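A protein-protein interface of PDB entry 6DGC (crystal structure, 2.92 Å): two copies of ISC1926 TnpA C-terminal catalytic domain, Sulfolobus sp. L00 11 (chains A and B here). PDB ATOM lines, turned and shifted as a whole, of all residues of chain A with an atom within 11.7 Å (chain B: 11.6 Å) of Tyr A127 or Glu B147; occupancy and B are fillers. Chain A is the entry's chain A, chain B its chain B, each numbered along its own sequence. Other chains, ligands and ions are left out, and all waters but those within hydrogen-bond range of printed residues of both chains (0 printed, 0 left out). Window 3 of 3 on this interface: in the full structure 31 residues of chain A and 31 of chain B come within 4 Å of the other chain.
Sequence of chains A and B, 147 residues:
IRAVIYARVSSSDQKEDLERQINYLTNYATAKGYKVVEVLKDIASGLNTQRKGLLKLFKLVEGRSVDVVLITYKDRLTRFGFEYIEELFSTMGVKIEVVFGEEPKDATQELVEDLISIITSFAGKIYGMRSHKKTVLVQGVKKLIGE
Of the printed residues of chain B, Phe A122 touches Leu B111 (3.2 Å) and Leu B115 (3.7 Å). Ala A123 touches none of the printed residues of chain B. No residue of chain B comes within 4 Å of Gly A124. Of the printed residues of chain B, Tyr A127 touches Ile B145 and Glu B147. No residue of chain B comes within 4 Å of Gly A128. No residue of chain B comes within 4 Å of Ser A131. No residue of chain B comes within 4 Å of Lys A133. No residue of chain B comes within 4 Å of Lys A134. No residue of chain B comes within 4 Å of Val A136. Of the printed residues of chain B, Val A141 touches Val B141 and Leu B144. Of the printed residues of chain A, Thr B108 touches Ile A126. Printed residues of chain A within 4 Å of Leu B111: Phe A122 (3.2 Å), Lys A125 (3.8 Å) and Ile A126 (3.6 Å). Of the printed residues of chain A, Ile B119 touches Ile A119. No residue of chain A comes within 4 Å of Lys B143. Printed residues of chain A within 4 Å of Glu B147: Tyr A127. The nearest residue of chain B that does not touch Tyr A127 is Leu B144 (5.0 Å).
Ile B119 touches its own counterpart, Ile A119. Val A141 touches its own counterpart, Val B141. 4 positions are printed for both chains.
Of the 24 printed residues of chain A, 8 touch a printed residue of chain B. Of the 22 printed residues of chain B, 9 touch a printed residue of chain A. Printed residues of chain B that touch a printed residue of chain A: Thr B108, Leu B111, Val B112, Leu B115, Ile B119, Val B141, Leu B144, Ile B145 and Glu B147. Hydrophobic or aromatic side chains of chain B that line the printed part of chain A: Leu B111, Val B112, Leu B115, Ile B119, Val B141, Leu B144 and Ile B145.
Among the printed residues, pairs that only touch across the chains: Ile A119 with Leu B115 (3.9 Å), Ile A119 with Ile B119 (3.7 Å), Phe A122 with Leu B111 (3.2 Å), Phe A122 with Leu B115 (3.7 Å), Lys A125 with Leu B111 (3.8 Å), Ile A126 with Thr B108 (3.9 Å), Ile A126 with Leu B111 (3.6 Å), Ile A126 with Val B112 (3.7 Å), Ile A126 with Leu B115 (3.8 Å), Tyr A127 with Glu B147 (3.7 Å), Leu A137 with Leu B144 (3.6 Å), Leu A137 with Ile B145 (3.8 Å), Gly A140 with Leu B144 (3.8 Å), Val A141 with Val B141 (3.7 Å) and Val A141 with Leu B144 (3.9 Å).
The backbone carbonyl oxygen of Ile B145 lies close to the side-chain hydroxyl of Tyr A127 (3.5 Å).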
ATOM      1  N   ILE A 118       3.412   1.187  27.783  1.00  0.00           N
ATOM      2  CA  ILE A 118       4.066   2.445  27.389  1.00  0.00           C
ATOM      3  C   ILE A 118       5.121   2.143  26.286  1.00  0.00           C
ATOM      4  O   ILE A 118       5.070   2.735  25.201  1.00  0.00           O
ATOM      5  CB  ILE A 118       4.650   3.235  28.616  1.00  0.00           C
ATOM      6  CG1 ILE A 118       3.547   3.697  29.583  1.00  0.00           C
ATOM      7  CG2 ILE A 118       5.506   4.439  28.160  1.00  0.00           C
ATOM      8  CD1 ILE A 118       4.042   3.949  31.030  1.00  0.00           C
ATOM      9  N   ILE A 119       6.029   1.182  26.566  1.00  0.00           N
ATOM     10  CA  ILE A 119       7.083   0.758  25.647  1.00  0.00           C
ATOM     11  C   ILE A 119       6.469   0.225  24.338  1.00  0.00           C
ATOM     12  O   ILE A 119       6.976   0.586  23.279  1.00  0.00           O
ATOM     13  CB  ILE A 119       8.091  -0.203  26.325  1.00  0.00           C
ATOM     14  CG1 ILE A 119       8.904   0.543  27.400  1.00  0.00           C
ATOM     15  CG2 ILE A 119       9.028  -0.864  25.314  1.00  0.00           C
ATOM     16  CD1 ILE A 119       9.368  -0.317  28.591  1.00  0.00           C
ATOM     17  N   THR A 120       5.349  -0.554  24.403  1.00  0.00           N
ATOM     18  CA  THR A 120       4.636  -1.071  23.221  1.00  0.00           C
ATOM     19  C   THR A 120       4.078   0.065  22.352  1.00  0.00           C
ATOM     20  O   THR A 120       4.254   0.035  21.128  1.00  0.00           O
ATOM     21  CB  THR A 120       3.519  -2.054  23.605  1.00  0.00           C
ATOM     22  OG1 THR A 120       4.062  -3.188  24.282  1.00  0.00           O
ATOM     23  N   SER A 121       3.412   1.067  22.984  1.00  0.00           N
ATOM     24  CA  SER A 121       2.853   2.198  22.253  1.00  0.00           C
ATOM     25  C   SER A 121       3.974   3.034  21.604  1.00  0.00           C
ATOM     26  O   SER A 121       3.922   3.275  20.391  1.00  0.00           O
ATOM     27  CB  SER A 121       1.984   3.057  23.160  1.00  0.00           C
ATOM     28  OG  SER A 121       2.783   3.826  24.042  1.00  0.00           O
ATOM     29  N   PHE A 122       5.003   3.424  22.404  1.00  0.00           N
ATOM     30  CA  PHE A 122       6.174   4.186  21.962  1.00  0.00           C
ATOM     31  C   PHE A 122       6.929   3.457  20.844  1.00  0.00           C
ATOM     32  O   PHE A 122       7.340   4.114  19.892  1.00  0.00           O
ATOM     33  CB  PHE A 122       7.117   4.464  23.131  1.00  0.00           C
ATOM     34  CG  PHE A 122       6.949   5.808  23.788  1.00  0.00           C
ATOM     35  CD1 PHE A 122       5.932   6.026  24.720  1.00  0.00           C
ATOM     36  CD2 PHE A 122       7.830   6.847  23.518  1.00  0.00           C
ATOM     37  CE1 PHE A 122       5.774   7.279  25.343  1.00  0.00           C
ATOM     38  CE2 PHE A 122       7.676   8.095  24.147  1.00  0.00           C
ATOM     39  CZ  PHE A 122       6.652   8.299  25.061  1.00  0.00           C
ATOM     40  N   ALA A 123       7.078   2.108  20.930  1.00  0.00           N
ATOM     41  CA  ALA A 123       7.739   1.300  19.889  1.00  0.00           C
ATOM     42  C   ALA A 123       7.016   1.438  18.551  1.00  0.00           C
ATOM     43  O   ALA A 123       7.656   1.525  17.509  1.00  0.00           O
ATOM     44  CB  ALA A 123       7.796  -0.159  20.299  1.00  0.00           C
ATOM     45  N   GLY A 124       5.687   1.499  18.616  1.00  0.00           N
ATOM     46  CA  GLY A 124       4.838   1.716  17.459  1.00  0.00           C
ATOM     47  C   GLY A 124       5.059   3.099  16.889  1.00  0.00           C
ATOM     48  O   GLY A 124       5.216   3.251  15.679  1.00  0.00           O
ATOM     49  N   LYS A 125       5.109   4.119  17.767  1.00  0.00           N
ATOM     50  CA  LYS A 125       5.346   5.508  17.369  1.00  0.00           C
ATOM     51  C   LYS A 125       6.755   5.690  16.732  1.00  0.00           C
ATOM     52  O   LYS A 125       6.878   6.382  15.716  1.00  0.00           O
ATOM     53  CB  LYS A 125       5.106   6.471  18.551  1.00  0.00           C
ATOM     54  N   ILE A 126       7.779   5.005  17.284  1.00  0.00           N
ATOM     55  CA  ILE A 126       9.173   5.074  16.832  1.00  0.00           C
ATOM     56  C   ILE A 126       9.427   4.257  15.562  1.00  0.00           C
ATOM     57  O   ILE A 126      10.019   4.785  14.622  1.00  0.00           O
ATOM     58  CB  ILE A 126      10.172   4.694  17.985  1.00  0.00           C
ATOM     59  CG1 ILE A 126      10.120   5.728  19.137  1.00  0.00           C
ATOM     60  CG2 ILE A 126      11.625   4.535  17.471  1.00  0.00           C
ATOM     61  CD1 ILE A 126      10.433   5.171  20.531  1.00  0.00           C
ATOM     62  N   TYR A 127       9.008   2.976  15.543  1.00  0.00           N
ATOM     63  CA  TYR A 127       9.283   2.034  14.446  1.00  0.00           C
ATOM     64  C   TYR A 127       8.097   1.715  13.512  1.00  0.00           C
ATOM     65  O   TYR A 127       8.315   1.466  12.334  1.00  0.00           O
ATOM     66  CB  TYR A 127       9.884   0.722  15.008  1.00  0.00           C
ATOM     67  CG  TYR A 127      11.106   0.927  15.888  1.00  0.00           C
ATOM     68  CD1 TYR A 127      12.326   1.322  15.340  1.00  0.00           C
ATOM     69  CD2 TYR A 127      11.042   0.725  17.267  1.00  0.00           C
ATOM     70  CE1 TYR A 127      13.449   1.526  16.141  1.00  0.00           C
ATOM     71  CE2 TYR A 127      12.163   0.917  18.080  1.00  0.00           C
ATOM     72  CZ  TYR A 127      13.369   1.312  17.507  1.00  0.00           C
ATOM     73  OH  TYR A 127      14.505   1.484  18.266  1.00  0.00           O
ATOM     74  N   GLY A 128       6.880   1.716  14.037  1.00  0.00           N
ATOM     75  CA  GLY A 128       5.668   1.402  13.282  1.00  0.00           C
ATOM     76  C   GLY A 128       4.730   0.523  14.086  1.00  0.00           C
ATOM     77  O   GLY A 128       5.167  -0.494  14.643  1.00  0.00           O
ATOM     78  N   MET A 129       3.429   0.919  14.163  1.00  0.00           N
ATOM     79  CA  MET A 129       2.371   0.225  14.925  1.00  0.00           C
ATOM     80  C   MET A 129       2.224  -1.283  14.568  1.00  0.00           C
ATOM     81  O   MET A 129       1.710  -2.053  15.392  1.00  0.00           O
ATOM     82  CB  MET A 129       1.021   0.965  14.833  1.00  0.00           C
ATOM     83  N   ARG A 130       2.716  -1.696  13.377  1.00  0.00           N
ATOM     84  CA  ARG A 130       2.712  -3.082  12.923  1.00  0.00           C
ATOM     85  C   ARG A 130       4.081  -3.418  12.270  1.00  0.00           C
ATOM     86  O   ARG A 130       4.141  -4.131  11.257  1.00  0.00           O
ATOM     87  CB  ARG A 130       1.519  -3.343  11.990  1.00  0.00           C
ATOM     88  N   SER A 131       5.186  -2.900  12.872  1.00  0.00           N
ATOM     89  CA  SER A 131       6.561  -3.093  12.387  1.00  0.00           C
ATOM     90  C   SER A 131       7.305  -4.230  13.063  1.00  0.00           C
ATOM     91  O   SER A 131       6.934  -4.624  14.169  1.00  0.00           O
ATOM     92  CB  SER A 131       7.364  -1.806  12.523  1.00  0.00           C
ATOM     93  N   HIS A 132       8.375  -4.746  12.400  1.00  0.00           N
ATOM     94  CA  HIS A 132       9.220  -5.838  12.906  1.00  0.00           C
ATOM     95  C   HIS A 132      10.115  -5.392  14.072  1.00  0.00           C
ATOM     96  O   HIS A 132      10.208  -6.101  15.076  1.00  0.00           O
ATOM     97  CB  HIS A 132      10.050  -6.472  11.780  1.00  0.00           C
ATOM     98  N   LYS A 133      10.750  -4.209  13.946  1.00  0.00           N
ATOM     99  CA  LYS A 133      11.613  -3.625  14.977  1.00  0.00           C
ATOM    100  C   LYS A 133      10.854  -3.315  16.302  1.00  0.00           C
ATOM    101  O   LYS A 133      11.462  -3.370  17.375  1.00  0.00           O
ATOM    102  CB  LYS A 133      12.336  -2.383  14.430  1.00  0.00           C
ATOM    103  N   LYS A 134       9.528  -3.014  16.217  1.00  0.00           N
ATOM    104  CA  LYS A 134       8.647  -2.764  17.367  1.00  0.00           C
ATOM    105  C   LYS A 134       8.558  -4.035  18.196  1.00  0.00           C
ATOM    106  O   LYS A 134       8.714  -3.973  19.413  1.00  0.00           O
ATOM    107  CB  LYS A 134       7.238  -2.328  16.922  1.00  0.00           C
ATOM    108  N   THR A 135       8.358  -5.192  17.526  1.00  0.00           N
ATOM    109  CA  THR A 135       8.277  -6.527  18.130  1.00  0.00           C
ATOM    110  C   THR A 135       9.605  -6.880  18.812  1.00  0.00           C
ATOM    111  O   THR A 135       9.592  -7.434  19.914  1.00  0.00           O
ATOM    112  CB  THR A 135       7.820  -7.558  17.076  1.00  0.00           C
ATOM    113  OG1 THR A 135       6.622  -7.080  16.461  1.00  0.00           O
ATOM    114  CG2 THR A 135       7.573  -8.943  17.663  1.00  0.00           C
ATOM    115  N   VAL A 136      10.739  -6.513  18.168  1.00  0.00           N
ATOM    116  CA  VAL A 136      12.115  -6.732  18.644  1.00  0.00           C
ATOM    117  C   VAL A 136      12.319  -6.090  20.032  1.00  0.00           C
ATOM    118  O   VAL A 136      12.751  -6.776  20.967  1.00  0.00           O
ATOM    119  CB  VAL A 136      13.154  -6.241  17.589  1.00  0.00           C
ATOM    120  CG1 VAL A 136      14.556  -6.117  18.177  1.00  0.00           C
ATOM    121  CG2 VAL A 136      13.164  -7.139  16.357  1.00  0.00           C
ATOM    122  N   LEU A 137      11.975  -4.788  20.161  1.00  0.00           N
ATOM    123  CA  LEU A 137      12.122  -4.034  21.403  1.00  0.00           C
ATOM    124  C   LEU A 137      11.203  -4.536  22.515  1.00  0.00           C
ATOM    125  O   LEU A 137      11.662  -4.692  23.648  1.00  0.00           O
ATOM    126  CB  LEU A 137      11.929  -2.524  21.150  1.00  0.00           C
ATOM    127  CG  LEU A 137      12.078  -1.564  22.347  1.00  0.00           C
ATOM    128  CD1 LEU A 137      13.521  -1.403  22.770  1.00  0.00           C
ATOM    129  CD2 LEU A 137      11.526  -0.211  22.008  1.00  0.00           C
ATOM    130  N   VAL A 138       9.926  -4.806  22.194  1.00  0.00           N
ATOM    131  CA  VAL A 138       8.940  -5.240  23.188  1.00  0.00           C
ATOM    132  C   VAL A 138       9.221  -6.668  23.690  1.00  0.00           C
ATOM    133  O   VAL A 138       8.986  -6.927  24.876  1.00  0.00           O
ATOM    134  CB  VAL A 138       7.454  -5.033  22.774  1.00  0.00           C
ATOM    135  CG1 VAL A 138       7.202  -3.579  22.424  1.00  0.00           C
ATOM    136  CG2 VAL A 138       7.026  -5.946  21.624  1.00  0.00           C
ATOM    137  N   GLN A 139       9.743  -7.573  22.814  1.00  0.00           N
ATOM    138  CA  GLN A 139      10.079  -8.941  23.208  1.00  0.00           C
ATOM    139  C   GLN A 139      11.344  -8.931  24.064  1.00  0.00           C
ATOM    140  O   GLN A 139      11.455  -9.723  24.999  1.00  0.00           O
ATOM    141  CB  GLN A 139      10.241  -9.856  21.990  1.00  0.00           C
ATOM    142  N   GLY A 140      12.256  -8.008  23.752  1.00  0.00           N
ATOM    143  CA  GLY A 140      13.515  -7.822  24.460  1.00  0.00           C
ATOM    144  C   GLY A 140      13.348  -7.253  25.855  1.00  0.00           C
ATOM    145  O   GLY A 140      13.951  -7.760  26.807  1.00  0.00           O
ATOM    146  N   VAL A 141      12.527  -6.191  25.982  1.00  0.00           N
ATOM    147  CA  VAL A 141      12.226  -5.517  27.253  1.00  0.00           C
ATOM    148  C   VAL A 141      11.520  -6.477  28.225  1.00  0.00           C
ATOM    149  O   VAL A 141      11.871  -6.510  29.410  1.00  0.00           O
ATOM    150  CB  VAL A 141      11.459  -4.193  27.037  1.00  0.00           C
ATOM    151  CG1 VAL A 141      10.792  -3.712  28.321  1.00  0.00           C
ATOM    152  CG2 VAL A 141      12.384  -3.115  26.473  1.00  0.00           C
ATOM    153  N   PRO B 104       4.200  14.256  14.976  1.00  0.00           N
ATOM    154  CA  PRO B 104       5.031  14.606  13.820  1.00  0.00           C
ATOM    155  C   PRO B 104       5.875  13.441  13.340  1.00  0.00           C
ATOM    156  O   PRO B 104       6.499  12.771  14.170  1.00  0.00           O
ATOM    157  CB  PRO B 104       5.919  15.757  14.320  1.00  0.00           C
ATOM    158  CG  PRO B 104       5.743  15.825  15.763  1.00  0.00           C
ATOM    159  CD  PRO B 104       4.493  15.095  16.153  1.00  0.00           C
ATOM    160  N   LYS B 105       5.935  13.219  12.000  1.00  0.00           N
ATOM    161  CA  LYS B 105       6.753  12.151  11.394  1.00  0.00           C
ATOM    162  C   LYS B 105       8.268  12.444  11.567  1.00  0.00           C
ATOM    163  O   LYS B 105       9.101  11.533  11.506  1.00  0.00           O
ATOM    164  CB  LYS B 105       6.383  11.943   9.919  1.00  0.00           C
ATOM    165  N   ASP B 106       8.591  13.728  11.839  1.00  0.00           N
ATOM    166  CA  ASP B 106       9.922  14.275  12.085  1.00  0.00           C
ATOM    167  C   ASP B 106      10.590  13.677  13.347  1.00  0.00           C
ATOM    168  O   ASP B 106      11.606  12.979  13.235  1.00  0.00           O
ATOM    169  CB  ASP B 106       9.817  15.811  12.206  1.00  0.00           C
ATOM    170  N   ALA B 107      10.001  13.956  14.543  1.00  0.00           N
ATOM    171  CA  ALA B 107      10.501  13.547  15.856  1.00  0.00           C
ATOM    172  C   ALA B 107      10.397  12.056  16.140  1.00  0.00           C
ATOM    173  O   ALA B 107       9.317  11.462  16.164  1.00  0.00           O
ATOM    174  CB  ALA B 107       9.832  14.349  16.955  1.00  0.00           C
ATOM    175  N   THR B 108      11.572  11.470  16.319  1.00  0.00           N
ATOM    176  CA  THR B 108      11.852  10.080  16.663  1.00  0.00           C
ATOM    177  C   THR B 108      12.840  10.185  17.814  1.00  0.00           C
ATOM    178  O   THR B 108      12.670   9.485  18.814  1.00  0.00           O
ATOM    179  CB  THR B 108      12.376   9.292  15.445  1.00  0.00           C
ATOM    180  OG1 THR B 108      11.340   9.242  14.455  1.00  0.00           O
ATOM    181  CG2 THR B 108      12.825   7.869  15.805  1.00  0.00           C
ATOM    182  N   GLN B 109      13.823  11.124  17.706  1.00  0.00           N
ATOM    183  CA  GLN B 109      14.794  11.417  18.760  1.00  0.00           C
ATOM    184  C   GLN B 109      14.056  11.900  20.011  1.00  0.00           C
ATOM    185  O   GLN B 109      14.468  11.528  21.112  1.00  0.00           O
ATOM    186  CB  GLN B 109      15.847  12.437  18.310  1.00  0.00           C
ATOM    187  N   GLU B 110      12.923  12.649  19.845  1.00  0.00           N
ATOM    188  CA  GLU B 110      12.104  13.117  20.981  1.00  0.00           C
ATOM    189  C   GLU B 110      11.356  11.956  21.632  1.00  0.00           C
ATOM    190  O   GLU B 110      11.281  11.895  22.852  1.00  0.00           O
ATOM    191  CB  GLU B 110      11.116  14.216  20.561  1.00  0.00           C
ATOM    192  CG  GLU B 110      10.772  15.181  21.676  1.00  0.00           C
ATOM    193  CD  GLU B 110       9.834  16.295  21.258  1.00  0.00           C
ATOM    194  OE1 GLU B 110       8.633  16.197  21.596  1.00  0.00           O
ATOM    195  OE2 GLU B 110      10.293  17.268  20.610  1.00  0.00           O
ATOM    196  N   LEU B 111      10.822  11.038  20.814  1.00  0.00           N
ATOM    197  CA  LEU B 111      10.115   9.856  21.282  1.00  0.00           C
ATOM    198  C   LEU B 111      11.075   8.895  22.000  1.00  0.00           C
ATOM    199  O   LEU B 111      10.685   8.292  23.014  1.00  0.00           O
ATOM    200  CB  LEU B 111       9.464   9.116  20.108  1.00  0.00           C
ATOM    201  CG  LEU B 111       8.153   9.641  19.569  1.00  0.00           C
ATOM    202  CD1 LEU B 111       7.920   9.091  18.192  1.00  0.00           C
ATOM    203  CD2 LEU B 111       6.978   9.219  20.438  1.00  0.00           C
ATOM    204  N   VAL B 112      12.310   8.723  21.465  1.00  0.00           N
ATOM    205  CA  VAL B 112      13.248   7.826  22.123  1.00  0.00           C
ATOM    206  C   VAL B 112      13.728   8.457  23.420  1.00  0.00           C
ATOM    207  O   VAL B 112      13.777   7.765  24.436  1.00  0.00           O
ATOM    208  CB  VAL B 112      14.413   7.248  21.267  1.00  0.00           C
ATOM    209  CG1 VAL B 112      13.896   6.417  20.100  1.00  0.00           C
ATOM    210  CG2 VAL B 112      15.377   8.325  20.791  1.00  0.00           C
ATOM    211  N   GLU B 113      14.002   9.775  23.415  1.00  0.00           N
ATOM    212  CA  GLU B 113      14.508  10.431  24.609  1.00  0.00           C
ATOM    213  C   GLU B 113      13.466  10.422  25.726  1.00  0.00           C
ATOM    214  O   GLU B 113      13.814  10.058  26.854  1.00  0.00           O
ATOM    215  CB  GLU B 113      15.136  11.811  24.314  1.00  0.00           C
ATOM    216  CG  GLU B 113      14.307  13.050  24.040  1.00  0.00           C
ATOM    217  CD  GLU B 113      15.177  14.242  23.650  1.00  0.00           C
ATOM    218  OE1 GLU B 113      16.219  14.471  24.310  1.00  0.00           O
ATOM    219  OE2 GLU B 113      14.820  14.945  22.676  1.00  0.00           O
ATOM    220  N   LEU B 115      11.059   8.186  26.013  1.00  0.00           N
ATOM    221  CA  LEU B 115      10.887   6.775  26.405  1.00  0.00           C
ATOM    222  C   LEU B 115      11.856   6.417  27.522  1.00  0.00           C
ATOM    223  O   LEU B 115      11.423   5.905  28.556  1.00  0.00           O
ATOM    224  CB  LEU B 115      11.045   5.824  25.191  1.00  0.00           C
ATOM    225  CG  LEU B 115      10.740   4.330  25.364  1.00  0.00           C
ATOM    226  CD1 LEU B 115       9.393   4.097  25.992  1.00  0.00           C
ATOM    227  CD2 LEU B 115      10.779   3.621  24.035  1.00  0.00           C
ATOM    228  N   ILE B 116      13.144   6.767  27.349  1.00  0.00           N
ATOM    229  CA  ILE B 116      14.181   6.525  28.347  1.00  0.00           C
ATOM    230  C   ILE B 116      13.796   7.141  29.685  1.00  0.00           C
ATOM    231  O   ILE B 116      13.644   6.395  30.644  1.00  0.00           O
ATOM    232  CB  ILE B 116      15.590   6.980  27.894  1.00  0.00           C
ATOM    233  CG1 ILE B 116      15.985   6.409  26.501  1.00  0.00           C
ATOM    234  CG2 ILE B 116      16.641   6.673  28.970  1.00  0.00           C
ATOM    235  CD1 ILE B 116      15.939   4.878  26.302  1.00  0.00           C
ATOM    236  N   ILE B 119      11.249   5.145  31.402  1.00  0.00           N
ATOM    237  CA  ILE B 119      11.844   3.870  31.814  1.00  0.00           C
ATOM    238  C   ILE B 119      12.717   4.058  33.051  1.00  0.00           C
ATOM    239  O   ILE B 119      12.564   3.285  33.997  1.00  0.00           O
ATOM    240  CB  ILE B 119      12.562   3.158  30.642  1.00  0.00           C
ATOM    241  CG1 ILE B 119      11.522   2.653  29.637  1.00  0.00           C
ATOM    242  CG2 ILE B 119      13.456   2.004  31.131  1.00  0.00           C
ATOM    243  CD1 ILE B 119      12.030   2.380  28.318  1.00  0.00           C
ATOM    244  N   GLN B 139      20.313   0.548  31.018  1.00  0.00           N
ATOM    245  CA  GLN B 139      21.491   0.372  30.167  1.00  0.00           C
ATOM    246  C   GLN B 139      21.162  -0.597  29.035  1.00  0.00           C
ATOM    247  O   GLN B 139      21.658  -0.420  27.922  1.00  0.00           O
ATOM    248  CB  GLN B 139      22.704  -0.122  30.969  1.00  0.00           C
ATOM    249  N   GLY B 140      20.305  -1.582  29.330  1.00  0.00           N
ATOM    250  CA  GLY B 140      19.858  -2.593  28.381  1.00  0.00           C
ATOM    251  C   GLY B 140      18.940  -2.049  27.305  1.00  0.00           C
ATOM    252  O   GLY B 140      19.129  -2.349  26.123  1.00  0.00           O
ATOM    253  N   VAL B 141      17.934  -1.243  27.717  1.00  0.00           N
ATOM    254  CA  VAL B 141      16.950  -0.613  26.831  1.00  0.00           C
ATOM    255  C   VAL B 141      17.645   0.347  25.866  1.00  0.00           C
ATOM    256  O   VAL B 141      17.324   0.340  24.671  1.00  0.00           O
ATOM    257  CB  VAL B 141      15.808   0.052  27.637  1.00  0.00           C
ATOM    258  CG1 VAL B 141      15.051   1.086  26.809  1.00  0.00           C
ATOM    259  CG2 VAL B 141      14.854  -1.001  28.199  1.00  0.00           C
ATOM    260  N   LYS B 142      18.628   1.131  26.380  1.00  0.00           N
ATOM    261  CA  LYS B 142      19.440   2.078  25.606  1.00  0.00           C
ATOM    262  C   LYS B 142      20.228   1.343  24.525  1.00  0.00           C
ATOM    263  O   LYS B 142      20.314   1.834  23.394  1.00  0.00           O
ATOM    264  CB  LYS B 142      20.391   2.866  26.522  1.00  0.00           C
ATOM    265  CG  LYS B 142      19.764   4.108  27.137  1.00  0.00           C
ATOM    266  CD  LYS B 142      20.786   4.959  27.869  1.00  0.00           C
ATOM    267  N   LYS B 143      20.768   0.146  24.868  1.00  0.00           N
ATOM    268  CA  LYS B 143      21.529  -0.721  23.964  1.00  0.00           C
ATOM    269  C   LYS B 143      20.607  -1.382  22.945  1.00  0.00           C
ATOM    270  O   LYS B 143      21.001  -1.535  21.788  1.00  0.00           O
ATOM    271  CB  LYS B 143      22.313  -1.778  24.751  1.00  0.00           C
ATOM    272  N   LEU B 144      19.381  -1.756  23.365  1.00  0.00           N
ATOM    273  CA  LEU B 144      18.369  -2.400  22.523  1.00  0.00           C
ATOM    274  C   LEU B 144      17.837  -1.486  21.409  1.00  0.00           C
ATOM    275  O   LEU B 144      17.547  -1.972  20.317  1.00  0.00           O
ATOM    276  CB  LEU B 144      17.219  -2.970  23.388  1.00  0.00           C
ATOM    277  CG  LEU B 144      16.185  -3.923  22.732  1.00  0.00           C
ATOM    278  CD1 LEU B 144      16.838  -4.969  21.842  1.00  0.00           C
ATOM    279  CD2 LEU B 144      15.307  -4.593  23.780  1.00  0.00           C
ATOM    280  N   ILE B 145      17.713  -0.176  21.673  1.00  0.00           N
ATOM    281  CA  ILE B 145      17.233   0.793  20.674  1.00  0.00           C
ATOM    282  C   ILE B 145      18.315   1.021  19.583  1.00  0.00           C
ATOM    283  O   ILE B 145      17.971   1.317  18.433  1.00  0.00           O
ATOM    284  CB  ILE B 145      16.690   2.103  21.336  1.00  0.00           C
ATOM    285  CG1 ILE B 145      15.462   1.791  22.209  1.00  0.00           C
ATOM    286  CG2 ILE B 145      16.367   3.202  20.306  1.00  0.00           C
ATOM    287  CD1 ILE B 145      15.274   2.699  23.355  1.00  0.00           C
ATOM    288  N   GLY B 146      19.588   0.815  19.949  1.00  0.00           N
ATOM    289  CA  GLY B 146      20.744   0.948  19.061  1.00  0.00           C
ATOM    290  C   GLY B 146      20.696   0.010  17.874  1.00  0.00           C
ATOM    291  O   GLY B 146      20.738   0.458  16.717  1.00  0.00           O
ATOM    292  N   GLU B 147      20.578  -1.312  18.187  1.00  0.00           N
ATOM    293  CA  GLU B 147      20.399  -2.450  17.273  1.00  0.00           C
ATOM    294  C   GLU B 147      21.228  -2.354  15.976  1.00  0.00           C
ATOM    295  O   GLU B 147      21.216  -3.264  15.143  1.00  0.00           O
ATOM    296  CB  GLU B 147      18.891  -2.672  16.966  1.00  0.00           C
ATOM    297  CG  GLU B 147      18.152  -1.443  16.437  1.00  0.00           C
ATOM    298  CD  GLU B 147      16.649  -1.497  16.242  1.00  0.00           C
ATOM    299  OE1 GLU B 147      16.182  -0.859  15.268  1.00  0.00           O
ATOM    300  OE2 GLU B 147      15.940  -2.117  17.072  1.00  0.00           O
